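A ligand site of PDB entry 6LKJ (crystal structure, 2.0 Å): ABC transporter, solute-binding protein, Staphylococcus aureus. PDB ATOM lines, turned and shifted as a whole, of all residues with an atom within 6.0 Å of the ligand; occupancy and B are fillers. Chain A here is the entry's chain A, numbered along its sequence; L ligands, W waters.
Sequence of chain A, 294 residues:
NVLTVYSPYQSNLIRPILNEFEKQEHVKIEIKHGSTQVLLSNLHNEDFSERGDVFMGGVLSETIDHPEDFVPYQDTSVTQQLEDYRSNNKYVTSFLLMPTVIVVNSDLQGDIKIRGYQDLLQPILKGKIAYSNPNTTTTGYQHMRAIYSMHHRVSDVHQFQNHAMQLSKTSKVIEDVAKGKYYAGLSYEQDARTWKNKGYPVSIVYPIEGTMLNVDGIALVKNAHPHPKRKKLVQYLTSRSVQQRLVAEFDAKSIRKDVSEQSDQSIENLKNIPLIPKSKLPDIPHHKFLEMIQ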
ATOM      1  N   PRO A   8     -16.544 -18.951  27.729  1.00  0.00           N
ATOM      2  CA  PRO A   8     -17.614 -19.598  26.961  1.00  0.00           C
ATOM      3  C   PRO A   8     -17.527 -21.121  26.953  1.00  0.00           C
ATOM      4  O   PRO A   8     -18.433 -21.776  26.426  1.00  0.00           O
ATOM      5  CB  PRO A   8     -17.430 -19.027  25.547  1.00  0.00           C
ATOM      6  CG  PRO A   8     -15.977 -18.684  25.484  1.00  0.00           C
ATOM      7  CD  PRO A   8     -15.605 -18.217  26.869  1.00  0.00           C
ATOM      8  N   TYR A   9     -16.461 -21.700  27.516  1.00  0.00           N
ATOM      9  CA  TYR A   9     -16.359 -23.149  27.621  1.00  0.00           C
ATOM     10  C   TYR A   9     -17.470 -23.705  28.502  1.00  0.00           C
ATOM     11  O   TYR A   9     -17.996 -23.012  29.380  1.00  0.00           O
ATOM     12  CB  TYR A   9     -15.007 -23.552  28.212  1.00  0.00           C
ATOM     13  CG  TYR A   9     -13.829 -23.438  27.290  1.00  0.00           C
ATOM     14  CD1 TYR A   9     -13.844 -23.998  26.022  1.00  0.00           C
ATOM     15  CD2 TYR A   9     -12.674 -22.773  27.699  1.00  0.00           C
ATOM     16  CE1 TYR A   9     -12.756 -23.894  25.172  1.00  0.00           C
ATOM     17  CE2 TYR A   9     -11.584 -22.674  26.862  1.00  0.00           C
ATOM     18  CZ  TYR A   9     -11.628 -23.227  25.601  1.00  0.00           C
ATOM     19  OH  TYR A   9     -10.541 -23.118  24.784  1.00  0.00           O
ATOM     20  N   GLY A  34     -21.250 -18.144  29.484  1.00  0.00           N
ATOM     21  CA  GLY A  34     -22.089 -17.478  28.514  1.00  0.00           C
ATOM     22  C   GLY A  34     -21.482 -17.565  27.128  1.00  0.00           C
ATOM     23  O   GLY A  34     -20.380 -18.059  26.943  1.00  0.00           O
ATOM     24  N   SER A  35     -22.265 -17.098  26.155  1.00  0.00           N
ATOM     25  CA  SER A  35     -21.749 -16.981  24.795  1.00  0.00           C
ATOM     26  C   SER A  35     -20.564 -16.016  24.766  1.00  0.00           C
ATOM     27  O   SER A  35     -20.484 -15.091  25.578  1.00  0.00           O
ATOM     28  CB  SER A  35     -22.845 -16.508  23.840  1.00  0.00           C
ATOM     29  OG  SER A  35     -23.967 -17.364  23.880  1.00  0.00           O
ATOM     30  N   THR A  36     -19.646 -16.251  23.836  1.00  0.00           N
ATOM     31  CA  THR A  36     -18.389 -15.498  23.804  1.00  0.00           C
ATOM     32  C   THR A  36     -18.641 -13.997  23.766  1.00  0.00           C
ATOM     33  O   THR A  36     -18.177 -13.249  24.642  1.00  0.00           O
ATOM     34  CB  THR A  36     -17.546 -15.929  22.607  1.00  0.00           C
ATOM     35  OG1 THR A  36     -17.243 -17.323  22.695  1.00  0.00           O
ATOM     36  CG2 THR A  36     -16.245 -15.127  22.572  1.00  0.00           C
ATOM     37  N   GLN A  37     -19.362 -13.527  22.746  1.00  0.00           N
ATOM     38  CA  GLN A  37     -19.584 -12.093  22.600  1.00  0.00           C
ATOM     39  C   GLN A  37     -20.497 -11.523  23.671  1.00  0.00           C
ATOM     40  O   GLN A  37     -20.415 -10.332  23.967  1.00  0.00           O
ATOM     41  CB  GLN A  37     -20.132 -11.790  21.211  1.00  0.00           C
ATOM     42  CG  GLN A  37     -19.141 -12.056  20.096  1.00  0.00           C
ATOM     43  CD  GLN A  37     -17.832 -11.309  20.277  1.00  0.00           C
ATOM     44  OE1 GLN A  37     -17.825 -10.112  20.563  1.00  0.00           O
ATOM     45  NE2 GLN A  37     -16.715 -12.011  20.107  1.00  0.00           N
ATOM     46  N   GLY A  57     -11.049 -19.050  26.487  1.00  0.00           N
ATOM     47  CA  GLY A  57     -11.982 -19.588  25.519  1.00  0.00           C
ATOM     48  C   GLY A  57     -12.400 -18.550  24.490  1.00  0.00           C
ATOM     49  O   GLY A  57     -12.286 -17.343  24.687  1.00  0.00           O
ATOM     50  N   GLY A  58     -12.887 -19.050  23.355  1.00  0.00           N
ATOM     51  CA  GLY A  58     -13.245 -18.193  22.244  1.00  0.00           C
ATOM     52  C   GLY A  58     -12.042 -17.790  21.419  1.00  0.00           C
ATOM     53  O   GLY A  58     -10.891 -17.835  21.860  1.00  0.00           O
ATOM     54  N   VAL A  59     -12.316 -17.388  20.175  1.00  0.00           N
ATOM     55  CA  VAL A  59     -11.254 -16.930  19.285  1.00  0.00           C
ATOM     56  C   VAL A  59     -10.924 -15.489  19.636  1.00  0.00           C
ATOM     57  O   VAL A  59     -11.244 -14.552  18.890  1.00  0.00           O
ATOM     58  CB  VAL A  59     -11.666 -17.091  17.806  1.00  0.00           C
ATOM     59  CG1 VAL A  59     -11.559 -18.552  17.397  1.00  0.00           C
ATOM     60  CG2 VAL A  59     -13.098 -16.605  17.575  1.00  0.00           C
ATOM     61  N   MET A  98      -9.291 -25.799  18.535  1.00  0.00           N
ATOM     62  CA  MET A  98     -10.634 -26.363  18.586  1.00  0.00           C
ATOM     63  C   MET A  98     -11.237 -26.392  17.187  1.00  0.00           C
ATOM     64  O   MET A  98     -11.685 -25.359  16.676  1.00  0.00           O
ATOM     65  CB  MET A  98     -11.530 -25.557  19.526  1.00  0.00           C
ATOM     66  CG  MET A  98     -12.868 -26.216  19.777  1.00  0.00           C
ATOM     67  SD  MET A  98     -12.704 -27.619  20.882  1.00  0.00           S
ATOM     68  CE  MET A  98     -12.390 -26.787  22.429  1.00  0.00           C
ATOM     69  N   THR A 100     -14.048 -26.620  14.562  1.00  0.00           N
ATOM     70  CA  THR A 100     -15.495 -26.579  14.425  1.00  0.00           C
ATOM     71  C   THR A 100     -15.947 -27.769  13.586  1.00  0.00           C
ATOM     72  O   THR A 100     -15.234 -28.200  12.676  1.00  0.00           O
ATOM     73  CB  THR A 100     -15.947 -25.262  13.781  1.00  0.00           C
ATOM     74  OG1 THR A 100     -15.334 -25.134  12.496  1.00  0.00           O
ATOM     75  CG2 THR A 100     -15.554 -24.076  14.644  1.00  0.00           C
ATOM     76  N   SER A 132     -25.880 -21.897  15.808  1.00  0.00           N
ATOM     77  CA  SER A 132     -25.998 -20.876  16.834  1.00  0.00           C
ATOM     78  C   SER A 132     -25.748 -19.491  16.251  1.00  0.00           C
ATOM     79  O   SER A 132     -25.102 -19.313  15.219  1.00  0.00           O
ATOM     80  CB  SER A 132     -25.024 -21.148  17.987  1.00  0.00           C
ATOM     81  OG  SER A 132     -23.676 -21.174  17.545  1.00  0.00           O
ATOM     82  N   THR A 136     -23.506 -13.525  18.382  1.00  0.00           N
ATOM     83  CA  THR A 136     -23.186 -13.626  19.801  1.00  0.00           C
ATOM     84  C   THR A 136     -22.216 -14.742  20.148  1.00  0.00           C
ATOM     85  O   THR A 136     -21.614 -14.696  21.230  1.00  0.00           O
ATOM     86  CB  THR A 136     -24.473 -13.845  20.612  1.00  0.00           C
ATOM     87  OG1 THR A 136     -25.148 -15.021  20.134  1.00  0.00           O
ATOM     88  CG2 THR A 136     -25.411 -12.652  20.483  1.00  0.00           C
ATOM     89  N   THR A 137     -22.038 -15.728  19.280  1.00  0.00           N
ATOM     90  CA  THR A 137     -21.253 -16.921  19.601  1.00  0.00           C
ATOM     91  C   THR A 137     -19.997 -16.994  18.755  1.00  0.00           C
ATOM     92  O   THR A 137     -19.938 -16.489  17.633  1.00  0.00           O
ATOM     93  CB  THR A 137     -22.076 -18.199  19.404  1.00  0.00           C
ATOM     94  OG1 THR A 137     -22.345 -18.375  18.006  1.00  0.00           O
ATOM     95  CG2 THR A 137     -23.393 -18.115  20.165  1.00  0.00           C
ATOM     96  N   THR A 138     -18.971 -17.645  19.318  1.00  0.00           N
ATOM     97  CA  THR A 138     -17.784 -17.968  18.535  1.00  0.00           C
ATOM     98  C   THR A 138     -18.086 -19.048  17.502  1.00  0.00           C
ATOM     99  O   THR A 138     -17.670 -18.943  16.344  1.00  0.00           O
ATOM    100  CB  THR A 138     -16.660 -18.426  19.461  1.00  0.00           C
ATOM    101  OG1 THR A 138     -16.095 -17.297  20.136  1.00  0.00           O
ATOM    102  CG2 THR A 138     -15.565 -19.150  18.677  1.00  0.00           C
ATOM    103  N   THR A 139     -18.844 -20.074  17.896  1.00  0.00           N
ATOM    104  CA  THR A 139     -19.082 -21.221  17.019  1.00  0.00           C
ATOM    105  C   THR A 139     -19.893 -20.824  15.799  1.00  0.00           C
ATOM    106  O   THR A 139     -19.544 -21.170  14.663  1.00  0.00           O
ATOM    107  CB  THR A 139     -19.777 -22.332  17.793  1.00  0.00           C
ATOM    108  OG1 THR A 139     -19.030 -22.620  18.989  1.00  0.00           O
ATOM    109  CG2 THR A 139     -19.886 -23.591  16.951  1.00  0.00           C
ATOM    110  N   GLY A 140     -21.001 -20.092  16.011  1.00  0.00           N
ATOM    111  CA  GLY A 140     -21.802 -19.657  14.874  1.00  0.00           C
ATOM    112  C   GLY A 140     -21.052 -18.726  13.951  1.00  0.00           C
ATOM    113  O   GLY A 140     -21.163 -18.828  12.727  1.00  0.00           O
ATOM    114  N   GLN A 142     -17.733 -18.562  13.507  1.00  0.00           N
ATOM    115  CA  GLN A 142     -16.683 -19.280  12.795  1.00  0.00           C
ATOM    116  C   GLN A 142     -17.250 -20.189  11.716  1.00  0.00           C
ATOM    117  O   GLN A 142     -16.616 -20.382  10.675  1.00  0.00           O
ATOM    118  CB  GLN A 142     -15.832 -20.083  13.784  1.00  0.00           C
ATOM    119  CG  GLN A 142     -14.920 -19.234  14.650  1.00  0.00           C
ATOM    120  CD  GLN A 142     -13.806 -18.582  13.853  1.00  0.00           C
ATOM    121  OE1 GLN A 142     -13.963 -17.481  13.333  1.00  0.00           O
ATOM    122  NE2 GLN A 142     -12.670 -19.276  13.752  1.00  0.00           N
ATOM    123  N   LYS A 169     -28.000 -20.385  21.772  1.00  0.00           N
ATOM    124  CA  LYS A 169     -26.825 -20.909  22.456  1.00  0.00           C
ATOM    125  C   LYS A 169     -26.174 -22.018  21.654  1.00  0.00           C
ATOM    126  O   LYS A 169     -26.855 -22.878  21.088  1.00  0.00           O
ATOM    127  CB  LYS A 169     -27.202 -21.422  23.845  1.00  0.00           C
ATOM    128  CG  LYS A 169     -27.872 -20.382  24.730  1.00  0.00           C
ATOM    129  CD  LYS A 169     -26.898 -19.287  25.123  1.00  0.00           C
ATOM    130  CE  LYS A 169     -25.818 -19.830  26.044  1.00  0.00           C
ATOM    131  NZ  LYS A 169     -24.994 -18.730  26.638  1.00  0.00           N
ATOM    132  N   THR A 170     -24.841 -21.996  21.610  1.00  0.00           N
ATOM    133  CA  THR A 170     -24.093 -23.006  20.880  1.00  0.00           C
ATOM    134  C   THR A 170     -24.356 -24.406  21.427  1.00  0.00           C
ATOM    135  O   THR A 170     -24.540 -25.364  20.656  1.00  0.00           O
ATOM    136  CB  THR A 170     -22.592 -22.700  20.917  1.00  0.00           C
ATOM    137  OG1 THR A 170     -22.321 -21.549  20.107  1.00  0.00           O
ATOM    138  CG2 THR A 170     -21.776 -23.876  20.417  1.00  0.00           C
ATOM    139  N   SER A 171     -24.380 -24.552  22.749  1.00  0.00           N
ATOM    140  CA  SER A 171     -24.557 -25.872  23.346  1.00  0.00           C
ATOM    141  C   SER A 171     -25.984 -26.386  23.176  1.00  0.00           C
ATOM    142  O   SER A 171     -26.216 -27.588  23.352  1.00  0.00           O
ATOM    143  CB  SER A 171     -24.177 -25.842  24.824  1.00  0.00           C
ATOM    144  OG  SER A 171     -22.769 -25.831  24.965  1.00  0.00           O
ATOM    145  N   SER A 187     -21.488 -27.361  15.343  1.00  0.00           N
ATOM    146  CA  SER A 187     -21.006 -27.370  16.721  1.00  0.00           C
ATOM    147  C   SER A 187     -19.477 -27.237  16.708  1.00  0.00           C
ATOM    148  O   SER A 187     -18.874 -26.725  15.754  1.00  0.00           O
ATOM    149  CB  SER A 187     -21.483 -28.642  17.428  1.00  0.00           C
ATOM    150  OG  SER A 187     -21.144 -28.623  18.800  1.00  0.00           O
ATOM    151  N   TYR A 188     -18.834 -27.691  17.783  1.00  0.00           N
ATOM    152  CA  TYR A 188     -17.382 -27.752  17.835  1.00  0.00           C
ATOM    153  C   TYR A 188     -16.972 -29.058  18.512  1.00  0.00           C
ATOM    154  O   TYR A 188     -17.790 -29.747  19.127  1.00  0.00           O
ATOM    155  CB  TYR A 188     -16.783 -26.530  18.550  1.00  0.00           C
ATOM    156  CG  TYR A 188     -17.188 -26.324  19.984  1.00  0.00           C
ATOM    157  CD1 TYR A 188     -18.411 -25.735  20.310  1.00  0.00           C
ATOM    158  CD2 TYR A 188     -16.343 -26.692  21.018  1.00  0.00           C
ATOM    159  CE1 TYR A 188     -18.771 -25.526  21.624  1.00  0.00           C
ATOM    160  CE2 TYR A 188     -16.702 -26.498  22.349  1.00  0.00           C
ATOM    161  CZ  TYR A 188     -17.924 -25.913  22.642  1.00  0.00           C
ATOM    162  OH  TYR A 188     -18.275 -25.707  23.953  1.00  0.00           O
ATOM    163  N   ASN A 214     -10.436 -23.241  15.223  1.00  0.00           N
ATOM    164  CA  ASN A 214     -10.404 -22.157  16.190  1.00  0.00           C
ATOM    165  C   ASN A 214      -9.104 -22.211  16.982  1.00  0.00           C
ATOM    166  O   ASN A 214      -8.708 -23.268  17.477  1.00  0.00           O
ATOM    167  CB  ASN A 214     -11.589 -22.251  17.152  1.00  0.00           C
ATOM    168  CG  ASN A 214     -12.917 -22.112  16.459  1.00  0.00           C
ATOM    169  OD1 ASN A 214     -12.990 -21.739  15.282  1.00  0.00           O
ATOM    170  ND2 ASN A 214     -13.995 -22.389  17.186  1.00  0.00           N
ATOM    171  N   ASP A 216      -8.248 -20.976  20.271  1.00  0.00           N
ATOM    172  CA  ASP A 216      -8.782 -20.413  21.506  1.00  0.00           C
ATOM    173  C   ASP A 216      -7.680 -19.681  22.273  1.00  0.00           C
ATOM    174  O   ASP A 216      -6.521 -20.095  22.273  1.00  0.00           O
ATOM    175  CB  ASP A 216      -9.388 -21.514  22.371  1.00  0.00           C
ATOM    176  CG  ASP A 216     -10.567 -22.194  21.712  1.00  0.00           C
ATOM    177  OD1 ASP A 216     -10.935 -21.815  20.581  1.00  0.00           O
ATOM    178  OD2 ASP A 216     -11.144 -23.112  22.338  1.00  0.00           O
HETATM  179  C1  LIG L   1     -15.931 -22.960  20.252  1.00  0.00           C
HETATM  180  C2  LIG L   1     -14.636 -22.336  20.755  1.00  0.00           C
HETATM  181  C3  LIG L   1     -14.538 -22.455  22.238  1.00  0.00           C
HETATM  182  C4  LIG L   1     -15.747 -21.866  22.915  1.00  0.00           C
HETATM  183  C5  LIG L   1     -17.038 -22.491  22.388  1.00  0.00           C
HETATM  184  C6  LIG L   1     -18.221 -21.854  23.035  1.00  0.00           C
HETATM  185  O1  LIG L   1     -16.040 -22.780  18.918  1.00  0.00           O
HETATM  186  O2  LIG L   1     -13.516 -23.004  20.144  1.00  0.00           O
HETATM  187  O3  LIG L   1     -13.365 -21.767  22.700  1.00  0.00           O
HETATM  188  O4  LIG L   1     -15.750 -20.460  22.656  1.00  0.00           O
HETATM  189  O5  LIG L   1     -17.135 -22.350  20.929  1.00  0.00           O
HETATM  190  O6  LIG L   1     -18.289 -20.527  22.684  1.00  0.00           O
HETATM  191  P1  LIG L   1     -19.682 -19.956  22.012  1.00  0.00           P
HETATM  192  O7  LIG L   1     -19.894 -20.576  20.658  1.00  0.00           O
HETATM  193  O8  LIG L   1     -19.570 -18.450  21.853  1.00  0.00           O
HETATM  194  O9  LIG L   1     -20.846 -20.276  22.903  1.00  0.00           O
HETATM  195  O   HOH W   1     -20.706 -21.257  25.304  1.00  0.00           O
HETATM  196  O   HOH W   2     -23.495 -20.146  23.265  1.00  0.00           O
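N of Gly 58 sits at hydrogen-bond distance from O3 of the ligand (2.8 Å). The side-chain hydroxyl (OG1) of Thr 139 is in hydrogen-bond range of an oxygen (O5) of the ligand (2.7 Å). N of Thr 139 is in hydrogen-bond range of O7 of the ligand, at 3.0 Å. An oxygen (O1) of the ligand is in hydrogen-bond range of the side-chain amide nitrogen (ND2) of Asn 214 (2.7 Å). An oxygen (O8) of the ligand sits at hydrogen-bond distance from the backbone NH (N) of Thr 36. The side-chain hydroxyl of Thr 170 is in hydrogen-bond range of an oxygen (O7) of the ligand. OD2 of Asp 216 sits at hydrogen-bond distance from O3 of the ligand, at 2.6 Å. An oxygen (O8) of the ligand lies within hydrogen-bond range of the backbone NH of Thr 138, 2.7 Å away. The side-chain hydroxyl (OG1) of Thr 36 lies within hydrogen-bond range of an oxygen (O8) of the ligand, 2.7 Å away.
Water W1 lies within hydrogen-bond range of the backbone carbonyl oxygen of Pro 8 and an oxygen (O9) of the ligand. Water W2 lies within hydrogen-bond range of an oxygen (O9) of the ligand, the backbone NH of Thr 170 and the side-chain hydroxyl of Ser 35.
Pro 8 touches the ligand. Tyr 9 touches the ligand (CE1 to O3, 3.3 Å). Ser 35 touches the ligand. Gly 57 touches the ligand (C to O3, 3.8 Å). Met 98 touches the ligand (CB to O2, 3.3 Å). Thr 137 touches the ligand. CZ of Tyr 188 touches C5 of the ligand, at 3.5 Å. Hydrophobic or aromatic side chains within 4 Å of the ligand: Pro 8, Tyr 9, Met 98 and Tyr 188. 14 residues have an atom within 4 Å of the ligand: Pro 8, Tyr 9, Ser 35, Thr 36, Gly 57, Gly 58, Met 98, Thr 137, Thr 138, Thr 139, Thr 170, Tyr 188, Asn 214 and Asp 216. Along chain A the residues within 4 Å of the ligand span positions 8 to 216.
The side-chain amide oxygen of Asn 214 sits at hydrogen-bond distance from the side-chain amide nitrogen of Gln 142. The backbone carbonyl oxygen of Asn 214 sits at hydrogen-bond distance from the backbone NH of Met 98 (2.8 Å). The backbone NH (N) of Gly 140 lies within hydrogen-bond range of the side-chain hydroxyl (OG1) of Thr 137, 3.0 Å away. The side-chain hydroxyl (OG1) of Thr 138 sits at hydrogen-bond distance from the side-chain hydroxyl (OG1) of Thr 36, at 2.8 Å. OG1 of Thr 170 is in hydrogen-bond range of OG of Ser 132. OG1 of Thr 137 sits at hydrogen-bond distance from OG of Ser 132, 3.1 Å away. OG of Ser 35 lies within hydrogen-bond range of NZ of Lys 169 (3.2 Å). The side-chain hydroxyl (OH) of Tyr 9 is in hydrogen-bond range of the side-chain carboxylate (OD2) of Asp 216 (2.5 Å).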
